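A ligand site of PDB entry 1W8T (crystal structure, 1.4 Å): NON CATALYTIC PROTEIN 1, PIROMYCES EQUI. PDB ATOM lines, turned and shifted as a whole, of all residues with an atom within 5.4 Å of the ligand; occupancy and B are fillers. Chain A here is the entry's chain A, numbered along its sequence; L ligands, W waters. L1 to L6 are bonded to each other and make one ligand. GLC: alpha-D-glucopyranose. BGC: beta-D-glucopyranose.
Water W10 lies within hydrogen-bond range of O3 of GLC L1 and OH of Tyr 46.
Water W7 bridges an oxygen (O2) of BGC L3 (2.7 Å) and the backbone carbonyl oxygen of Lys 45 (3.1 Å).
Water W12 lies within hydrogen-bond range of OD1 of Asp 83 and O6 of BGC L5.
Water W11 lies within hydrogen-bond range of an oxygen (O3) of BGC L5 (2.8 Å), the backbone carbonyl oxygen (O) of Gly 25 (2.8 Å) and the backbone carbonyl oxygen (O) of Trp 24 (3.4 Å).
Water W14 bridges the side-chain amide oxygen (OE1) of Gln 116 (2.7 Å) and an oxygen (O3) of BGC L2 (2.8 Å).
Water W6 lies within hydrogen-bond range of OH of Tyr 46 and O5 of GLC L1.
Residues that only touch the ligand: Gly 25, Trp 26, Tyr 46, Lys 85 and Pro 119.
Hydrophobic or aromatic side chains that line the ligand: Trp 24, Trp 26 and Tyr 46.
Ten residues have an atom within 4 Å of the ligand: Trp 24, Gly 25, Trp 26, Tyr 46, Glu 78, Lys 85, Arg 112, Gln 116, Ala 118 and Pro 119.
The nearest printed residue that does not touch the ligand is Asp 83 (4.04 Å).
The side-chain carboxylate (OE2) of Glu 78 lies within salt-bridge range of the guanidinium group (NH2) of Arg 112.
OE2 of Glu 78 lies close to OD2 of Asp 114 (2.4 Å).
The backbone carbonyl oxygen of Tyr 46 is in hydrogen-bond range of the side-chain amide nitrogen of Gln 116 (2.9 Å).
NH2 of Arg 112 sits at hydrogen-bond distance from O of Trp 24 (3.4 Å).
The indole nitrogen (NE1) of Trp 26 lies within hydrogen-bond range of the backbone carbonyl oxygen (O) of Tyr 46 (3.0 Å).
O6 of BGC L3 is in hydrogen-bond range of OE1 of Gln 116 (2.8 Å).
O of Trp 24 lies within hydrogen-bond range of O2 of BGC L5, at 2.7 Å.
The backbone carbonyl oxygen of Ala 118 sits at hydrogen-bond distance from an oxygen (O6) of GLC L1.
O4 of BGC L4 sits at hydrogen-bond distance from NH2 of Arg 112, at 3.0 Å.
O3 of BGC L4 lies within hydrogen-bond range of OE1 of Glu 78, 2.7 Å away.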
ATOM      1  N   TRP A  24     -17.675  15.247 -12.526  1.00  0.00           N
ATOM      2  CA  TRP A  24     -16.799  15.984 -11.608  1.00  0.00           C
ATOM      3  C   TRP A  24     -16.741  15.265 -10.254  1.00  0.00           C
ATOM      4  O   TRP A  24     -16.506  15.867  -9.211  1.00  0.00           O
ATOM      5  CB  TRP A  24     -17.316  17.410 -11.421  1.00  0.00           C
ATOM      6  CG  TRP A  24     -17.068  18.347 -12.565  1.00  0.00           C
ATOM      7  CD1 TRP A  24     -16.818  18.032 -13.881  1.00  0.00           C
ATOM      8  CD2 TRP A  24     -17.069  19.781 -12.488  1.00  0.00           C
ATOM      9  NE1 TRP A  24     -16.648  19.183 -14.604  1.00  0.00           N
ATOM     10  CE2 TRP A  24     -16.815  20.270 -13.787  1.00  0.00           C
ATOM     11  CE3 TRP A  24     -17.244  20.705 -11.439  1.00  0.00           C
ATOM     12  CZ2 TRP A  24     -16.714  21.637 -14.079  1.00  0.00           C
ATOM     13  CZ3 TRP A  24     -17.152  22.059 -11.750  1.00  0.00           C
ATOM     14  CH2 TRP A  24     -16.890  22.502 -13.063  1.00  0.00           C
ATOM     15  N   GLY A  25     -16.933  13.945 -10.291  1.00  0.00           N
ATOM     16  CA  GLY A  25     -16.909  13.130  -9.100  1.00  0.00           C
ATOM     17  C   GLY A  25     -15.528  12.944  -8.524  1.00  0.00           C
ATOM     18  O   GLY A  25     -14.518  13.501  -9.005  1.00  0.00           O
ATOM     19  N   TRP A  26     -15.484  12.182  -7.456  1.00  0.00           N
ATOM     20  CA  TRP A  26     -14.246  12.007  -6.713  1.00  0.00           C
ATOM     21  C   TRP A  26     -14.343  10.670  -6.006  1.00  0.00           C
ATOM     22  O   TRP A  26     -15.420  10.191  -5.622  1.00  0.00           O
ATOM     23  CB  TRP A  26     -14.028  13.146  -5.740  1.00  0.00           C
ATOM     24  CG  TRP A  26     -15.085  13.268  -4.691  1.00  0.00           C
ATOM     25  CD1 TRP A  26     -15.047  12.707  -3.431  1.00  0.00           C
ATOM     26  CD2 TRP A  26     -16.366  13.945  -4.756  1.00  0.00           C
ATOM     27  NE1 TRP A  26     -16.185  12.996  -2.734  1.00  0.00           N
ATOM     28  CE2 TRP A  26     -17.021  13.751  -3.533  1.00  0.00           C
ATOM     29  CE3 TRP A  26     -17.021  14.675  -5.739  1.00  0.00           C
ATOM     30  CZ2 TRP A  26     -18.280  14.273  -3.259  1.00  0.00           C
ATOM     31  CZ3 TRP A  26     -18.253  15.216  -5.459  1.00  0.00           C
ATOM     32  CH2 TRP A  26     -18.883  15.010  -4.239  1.00  0.00           C
ATOM     33  N   LYS A  45     -13.008   7.441   1.232  1.00  0.00           N
ATOM     34  CA  LYS A  45     -12.952   8.654   0.428  1.00  0.00           C
ATOM     35  C   LYS A  45     -14.295   9.418   0.415  1.00  0.00           C
ATOM     36  O   LYS A  45     -14.354  10.549  -0.049  1.00  0.00           O
ATOM     37  CB  LYS A  45     -12.527   8.312  -0.985  1.00  0.00           C
ATOM     38  CG  LYS A  45     -11.087   7.767  -1.081  1.00  0.00           C
ATOM     39  CD  LYS A  45     -10.024   8.814  -0.824  1.00  0.00           C
ATOM     40  CE  LYS A  45      -8.639   8.181  -0.808  1.00  0.00           C
ATOM     41  NZ  LYS A  45      -7.698   8.972   0.091  1.00  0.00           N
ATOM     42  N   TYR A  46     -15.355   8.819   0.926  1.00  0.00           N
ATOM     43  CA  TYR A  46     -16.703   9.368   0.820  1.00  0.00           C
ATOM     44  C   TYR A  46     -16.980   9.806  -0.618  1.00  0.00           C
ATOM     45  O   TYR A  46     -17.421  10.951  -0.858  1.00  0.00           O
ATOM     46  CB  TYR A  46     -16.902  10.488   1.845  1.00  0.00           C
ATOM     47  CG  TYR A  46     -16.645  10.029   3.269  1.00  0.00           C
ATOM     48  CD1 TYR A  46     -15.351   9.997   3.799  1.00  0.00           C
ATOM     49  CD2 TYR A  46     -17.685   9.599   4.067  1.00  0.00           C
ATOM     50  CE1 TYR A  46     -15.123   9.570   5.099  1.00  0.00           C
ATOM     51  CE2 TYR A  46     -17.476   9.134   5.369  1.00  0.00           C
ATOM     52  CZ  TYR A  46     -16.184   9.133   5.879  1.00  0.00           C
ATOM     53  OH  TYR A  46     -15.950   8.701   7.184  1.00  0.00           O
ATOM     54  N   LEU A  76     -27.034  15.107  -3.475  1.00  0.00           N
ATOM     55  CA  LEU A  76     -26.786  16.561  -3.397  1.00  0.00           C
ATOM     56  C   LEU A  76     -26.943  17.190  -4.744  1.00  0.00           C
ATOM     57  O   LEU A  76     -26.821  16.526  -5.785  1.00  0.00           O
ATOM     58  CB  LEU A  76     -25.392  16.901  -2.834  1.00  0.00           C
ATOM     59  CG  LEU A  76     -25.063  16.253  -1.492  1.00  0.00           C
ATOM     60  CD1 LEU A  76     -24.322  14.963  -1.704  1.00  0.00           C
ATOM     61  CD2 LEU A  76     -24.224  17.232  -0.645  1.00  0.00           C
ATOM     62  N   GLU A  78     -25.430  20.946  -6.701  1.00  0.00           N
ATOM     63  CA  GLU A  78     -24.482  22.061  -6.502  1.00  0.00           C
ATOM     64  C   GLU A  78     -24.629  23.061  -7.629  1.00  0.00           C
ATOM     65  O   GLU A  78     -24.970  22.724  -8.739  1.00  0.00           O
ATOM     66  CB  GLU A  78     -23.009  21.611  -6.436  1.00  0.00           C
ATOM     67  CG  GLU A  78     -22.743  20.322  -5.671  1.00  0.00           C
ATOM     68  CD  GLU A  78     -21.261  20.012  -5.577  1.00  0.00           C
ATOM     69  OE1 GLU A  78     -20.454  20.926  -5.473  1.00  0.00           O
ATOM     70  OE2 GLU A  78     -20.876  18.826  -5.596  1.00  0.00           O
ATOM     71  N   ASP A  83     -20.107  27.824  -6.155  1.00  0.00           N
ATOM     72  CA  ASP A  83     -19.551  26.741  -5.339  1.00  0.00           C
ATOM     73  C   ASP A  83     -20.392  26.488  -4.098  1.00  0.00           C
ATOM     74  O   ASP A  83     -19.907  26.444  -2.992  1.00  0.00           O
ATOM     75  CB  ASP A  83     -18.086  26.975  -4.968  1.00  0.00           C
ATOM     76  CG  ASP A  83     -17.437  25.759  -4.372  1.00  0.00           C
ATOM     77  OD1 ASP A  83     -17.864  24.641  -4.727  1.00  0.00           O
ATOM     78  OD2 ASP A  83     -16.515  25.838  -3.529  1.00  0.00           O
ATOM     79  N   LYS A  85     -23.350  23.945  -2.364  1.00  0.00           N
ATOM     80  CA  LYS A  85     -23.935  22.606  -2.356  1.00  0.00           C
ATOM     81  C   LYS A  85     -25.188  22.568  -1.510  1.00  0.00           C
ATOM     82  O   LYS A  85     -25.401  23.433  -0.620  1.00  0.00           O
ATOM     83  CB  LYS A  85     -22.927  21.578  -1.874  1.00  0.00           C
ATOM     84  CG  LYS A  85     -22.738  21.535  -0.426  1.00  0.00           C
ATOM     85  CD  LYS A  85     -21.657  20.548  -0.047  1.00  0.00           C
ATOM     86  CE  LYS A  85     -21.538  20.431   1.458  1.00  0.00           C
ATOM     87  NZ  LYS A  85     -22.833  19.910   2.004  1.00  0.00           N
ATOM     88  N   ARG A 112     -24.782  20.608 -11.018  1.00  0.00           N
ATOM     89  CA  ARG A 112     -24.148  19.349 -10.591  1.00  0.00           C
ATOM     90  C   ARG A 112     -25.162  18.568  -9.770  1.00  0.00           C
ATOM     91  O   ARG A 112     -25.841  19.093  -8.919  1.00  0.00           O
ATOM     92  CB  ARG A 112     -22.907  19.619  -9.737  1.00  0.00           C
ATOM     93  CG  ARG A 112     -21.768  20.258 -10.506  1.00  0.00           C
ATOM     94  CD  ARG A 112     -20.584  20.657  -9.669  1.00  0.00           C
ATOM     95  NE  ARG A 112     -19.980  19.479  -9.078  1.00  0.00           N
ATOM     96  CZ  ARG A 112     -18.930  19.457  -8.282  1.00  0.00           C
ATOM     97  NH1 ARG A 112     -18.301  20.557  -7.946  1.00  0.00           N
ATOM     98  NH2 ARG A 112     -18.479  18.314  -7.805  1.00  0.00           N
ATOM     99  N   ASP A 114     -25.143  15.049  -7.490  1.00  0.00           N
ATOM    100  CA  ASP A 114     -24.181  14.159  -6.815  1.00  0.00           C
ATOM    101  C   ASP A 114     -24.904  12.991  -6.149  1.00  0.00           C
ATOM    102  O   ASP A 114     -25.946  13.148  -5.495  1.00  0.00           O
ATOM    103  CB  ASP A 114     -23.448  14.903  -5.716  1.00  0.00           C
ATOM    104  CG  ASP A 114     -22.748  16.149  -6.146  1.00  0.00           C
ATOM    105  OD1 ASP A 114     -22.599  16.407  -7.355  1.00  0.00           O
ATOM    106  OD2 ASP A 114     -22.353  16.930  -5.190  1.00  0.00           O
ATOM    107  N   GLN A 116     -23.493  10.271  -3.458  1.00  0.00           N
ATOM    108  CA  GLN A 116     -22.323  10.113  -2.617  1.00  0.00           C
ATOM    109  C   GLN A 116     -22.468   8.944  -1.655  1.00  0.00           C
ATOM    110  O   GLN A 116     -23.492   8.710  -1.020  1.00  0.00           O
ATOM    111  CB  GLN A 116     -22.051  11.410  -1.860  1.00  0.00           C
ATOM    112  CG  GLN A 116     -20.813  11.361  -0.961  1.00  0.00           C
ATOM    113  CD  GLN A 116     -20.532  12.673  -0.267  1.00  0.00           C
ATOM    114  OE1 GLN A 116     -21.441  13.483  -0.078  1.00  0.00           O
ATOM    115  NE2 GLN A 116     -19.293  12.853   0.169  1.00  0.00           N
ATOM    116  N   ALA A 118     -22.170   8.097   1.516  1.00  0.00           N
ATOM    117  CA  ALA A 118     -22.201   8.814   2.790  1.00  0.00           C
ATOM    118  C   ALA A 118     -21.383   8.143   3.908  1.00  0.00           C
ATOM    119  O   ALA A 118     -20.711   8.889   4.658  1.00  0.00           O
ATOM    120  CB  ALA A 118     -23.622   9.048   3.244  1.00  0.00           C
ATOM    121  N   PRO A 119     -21.485   6.845   4.095  1.00  0.00           N
ATOM    122  CA  PRO A 119     -20.713   6.188   5.171  1.00  0.00           C
ATOM    123  C   PRO A 119     -19.253   6.090   4.891  1.00  0.00           C
ATOM    124  O   PRO A 119     -18.486   5.817   5.838  1.00  0.00           O
ATOM    125  CB  PRO A 119     -21.304   4.775   5.239  1.00  0.00           C
ATOM    126  CG  PRO A 119     -22.626   4.900   4.536  1.00  0.00           C
ATOM    127  CD  PRO A 119     -22.362   5.881   3.413  1.00  0.00           C
ATOM    128  N   GLY A 120     -18.797   6.251   3.658  1.00  0.00           N
ATOM    129  CA  GLY A 120     -17.385   6.141   3.350  1.00  0.00           C
ATOM    130  C   GLY A 120     -16.851   4.723   3.513  1.00  0.00           C
ATOM    131  O   GLY A 120     -15.612   4.555   3.639  1.00  0.00           O
HETATM  132  C1  GLC L   1     -19.246  10.054  11.024  1.00  0.00           C
HETATM  133  C2  GLC L   1     -17.897  10.657  10.755  1.00  0.00           C
HETATM  134  C3  GLC L   1     -18.196  11.823   9.804  1.00  0.00           C
HETATM  135  C4  GLC L   1     -19.045  11.412   8.593  1.00  0.00           C
HETATM  136  C5  GLC L   1     -20.302  10.653   9.048  1.00  0.00           C
HETATM  137  C6  GLC L   1     -21.149  10.210   7.857  1.00  0.00           C
HETATM  138  O1  GLC L   1     -20.034  10.745  11.942  1.00  0.00           O
HETATM  139  O2  GLC L   1     -17.228  11.124  11.946  1.00  0.00           O
HETATM  140  O3  GLC L   1     -16.959  12.367   9.432  1.00  0.00           O
HETATM  141  O4  GLC L   1     -19.433  12.622   7.947  1.00  0.00           O
HETATM  142  O5  GLC L   1     -19.904   9.541   9.850  1.00  0.00           O
HETATM  143  O6  GLC L   1     -20.432   9.138   7.296  1.00  0.00           O
HETATM  144  C2  BGC L   2     -19.956  13.804   5.951  1.00  0.00           C
HETATM  145  C3  BGC L   2     -19.509  14.023   4.513  1.00  0.00           C
HETATM  146  C4  BGC L   2     -18.014  14.183   4.399  1.00  0.00           C
HETATM  147  C5  BGC L   2     -17.286  13.098   5.192  1.00  0.00           C
HETATM  148  C6  BGC L   2     -15.809  13.381   5.313  1.00  0.00           C
HETATM  149  C1  BGC L   2     -19.120  12.676   6.551  1.00  0.00           C
HETATM  150  O2  BGC L   2     -21.313  13.418   5.952  1.00  0.00           O
HETATM  151  O3  BGC L   2     -20.198  15.146   3.977  1.00  0.00           O
HETATM  152  O4  BGC L   2     -17.583  14.014   3.061  1.00  0.00           O
HETATM  153  O5  BGC L   2     -17.800  13.060   6.504  1.00  0.00           O
HETATM  154  O6  BGC L   2     -15.680  14.658   5.852  1.00  0.00           O
HETATM  155  C2  BGC L   3     -16.239  15.146   1.472  1.00  0.00           C
HETATM  156  C3  BGC L   3     -16.113  16.346   0.555  1.00  0.00           C
HETATM  157  C4  BGC L   3     -17.475  16.625  -0.125  1.00  0.00           C
HETATM  158  C5  BGC L   3     -18.589  16.669   0.898  1.00  0.00           C
HETATM  159  C6  BGC L   3     -19.983  16.857   0.337  1.00  0.00           C
HETATM  160  C1  BGC L   3     -17.439  15.246   2.383  1.00  0.00           C
HETATM  161  O2  BGC L   3     -15.045  14.996   2.280  1.00  0.00           O
HETATM  162  O3  BGC L   3     -15.110  16.126  -0.392  1.00  0.00           O
HETATM  163  O4  BGC L   3     -17.486  17.907  -0.772  1.00  0.00           O
HETATM  164  O5  BGC L   3     -18.607  15.443   1.605  1.00  0.00           O
HETATM  165  O6  BGC L   3     -20.251  15.966  -0.705  1.00  0.00           O
HETATM  166  C2  BGC L   4     -17.793  19.172  -2.764  1.00  0.00           C
HETATM  167  C3  BGC L   4     -17.603  19.076  -4.261  1.00  0.00           C
HETATM  168  C4  BGC L   4     -16.178  18.669  -4.619  1.00  0.00           C
HETATM  169  C5  BGC L   4     -15.800  17.410  -3.840  1.00  0.00           C
HETATM  170  C6  BGC L   4     -14.392  16.931  -4.095  1.00  0.00           C
HETATM  171  C1  BGC L   4     -17.333  17.842  -2.158  1.00  0.00           C
HETATM  172  O2  BGC L   4     -19.147  19.456  -2.432  1.00  0.00           O
HETATM  173  O3  BGC L   4     -17.894  20.309  -4.919  1.00  0.00           O
HETATM  174  O4  BGC L   4     -16.098  18.415  -6.027  1.00  0.00           O
HETATM  175  O5  BGC L   4     -16.004  17.598  -2.464  1.00  0.00           O
HETATM  176  O6  BGC L   4     -13.467  17.925  -3.697  1.00  0.00           O
HETATM  177  C2  BGC L   5     -14.858  18.203  -7.988  1.00  0.00           C
HETATM  178  C3  BGC L   5     -13.871  18.889  -8.911  1.00  0.00           C
HETATM  179  C4  BGC L   5     -14.151  20.371  -9.074  1.00  0.00           C
HETATM  180  C5  BGC L   5     -14.312  21.000  -7.714  1.00  0.00           C
HETATM  181  C6  BGC L   5     -14.756  22.465  -7.844  1.00  0.00           C
HETATM  182  C1  BGC L   5     -14.990  18.970  -6.704  1.00  0.00           C
HETATM  183  O2  BGC L   5     -14.476  16.849  -7.768  1.00  0.00           O
HETATM  184  O3  BGC L   5     -13.845  18.208 -10.182  1.00  0.00           O
HETATM  185  O4  BGC L   5     -13.051  21.018  -9.731  1.00  0.00           O
HETATM  186  O5  BGC L   5     -15.337  20.309  -6.971  1.00  0.00           O
HETATM  187  O6  BGC L   5     -14.625  23.118  -6.605  1.00  0.00           O
HETATM  188  C2  BGC L   6     -12.255  22.402 -11.533  1.00  0.00           C
HETATM  189  C3  BGC L   6     -12.365  22.627 -13.021  1.00  0.00           C
HETATM  190  C4  BGC L   6     -12.257  21.315 -13.774  1.00  0.00           C
HETATM  191  C5  BGC L   6     -13.259  20.299 -13.229  1.00  0.00           C
HETATM  192  C6  BGC L   6     -13.173  18.938 -13.902  1.00  0.00           C
HETATM  193  C1  BGC L   6     -13.258  21.324 -11.088  1.00  0.00           C
HETATM  194  O2  BGC L   6     -12.521  23.573 -10.777  1.00  0.00           O
HETATM  195  O3  BGC L   6     -11.318  23.484 -13.434  1.00  0.00           O
HETATM  196  O4  BGC L   6     -12.531  21.521 -15.148  1.00  0.00           O
HETATM  197  O5  BGC L   6     -13.070  20.155 -11.833  1.00  0.00           O
HETATM  198  O6  BGC L   6     -11.935  18.320 -13.614  1.00  0.00           O
HETATM  199  O   HOH W   1     -20.980  17.589  -2.748  1.00  0.00           O
HETATM  200  O   HOH W   2     -18.615  20.434   0.226  1.00  0.00           O
HETATM  201  O   HOH W   3     -21.866   7.620   8.958  1.00  0.00           O
HETATM  202  O   HOH W   4     -22.689  13.522   8.333  1.00  0.00           O
HETATM  203  O   HOH W   5     -11.874  15.942  -7.334  1.00  0.00           O
HETATM  204  O   HOH W   6     -17.831   7.758   8.741  1.00  0.00           O
HETATM  205  O   HOH W   7     -13.609  12.755   1.940  1.00  0.00           O
HETATM  206  O   HOH W   8     -22.217   9.451  12.667  1.00  0.00           O
HETATM  207  O   HOH W   9     -13.797  19.619  -1.519  1.00  0.00           O
HETATM  208  O   HOH W  10     -15.105  10.625   8.821  1.00  0.00           O
HETATM  209  O   HOH W  11     -13.513  15.488 -10.686  1.00  0.00           O
HETATM  210  O   HOH W  12     -16.288  22.511  -4.505  1.00  0.00           O
HETATM  211  O   HOH W  13     -14.865  25.038 -11.028  1.00  0.00           O
HETATM  212  O   HOH W  14     -22.333  14.576   2.231  1.00  0.00           O
HETATM  213  O   HOH W  15     -19.617  17.800   4.424  1.00  0.00           O
HETATM  214  O   HOH W  16     -15.035  25.805  -7.199  1.00  0.00           O
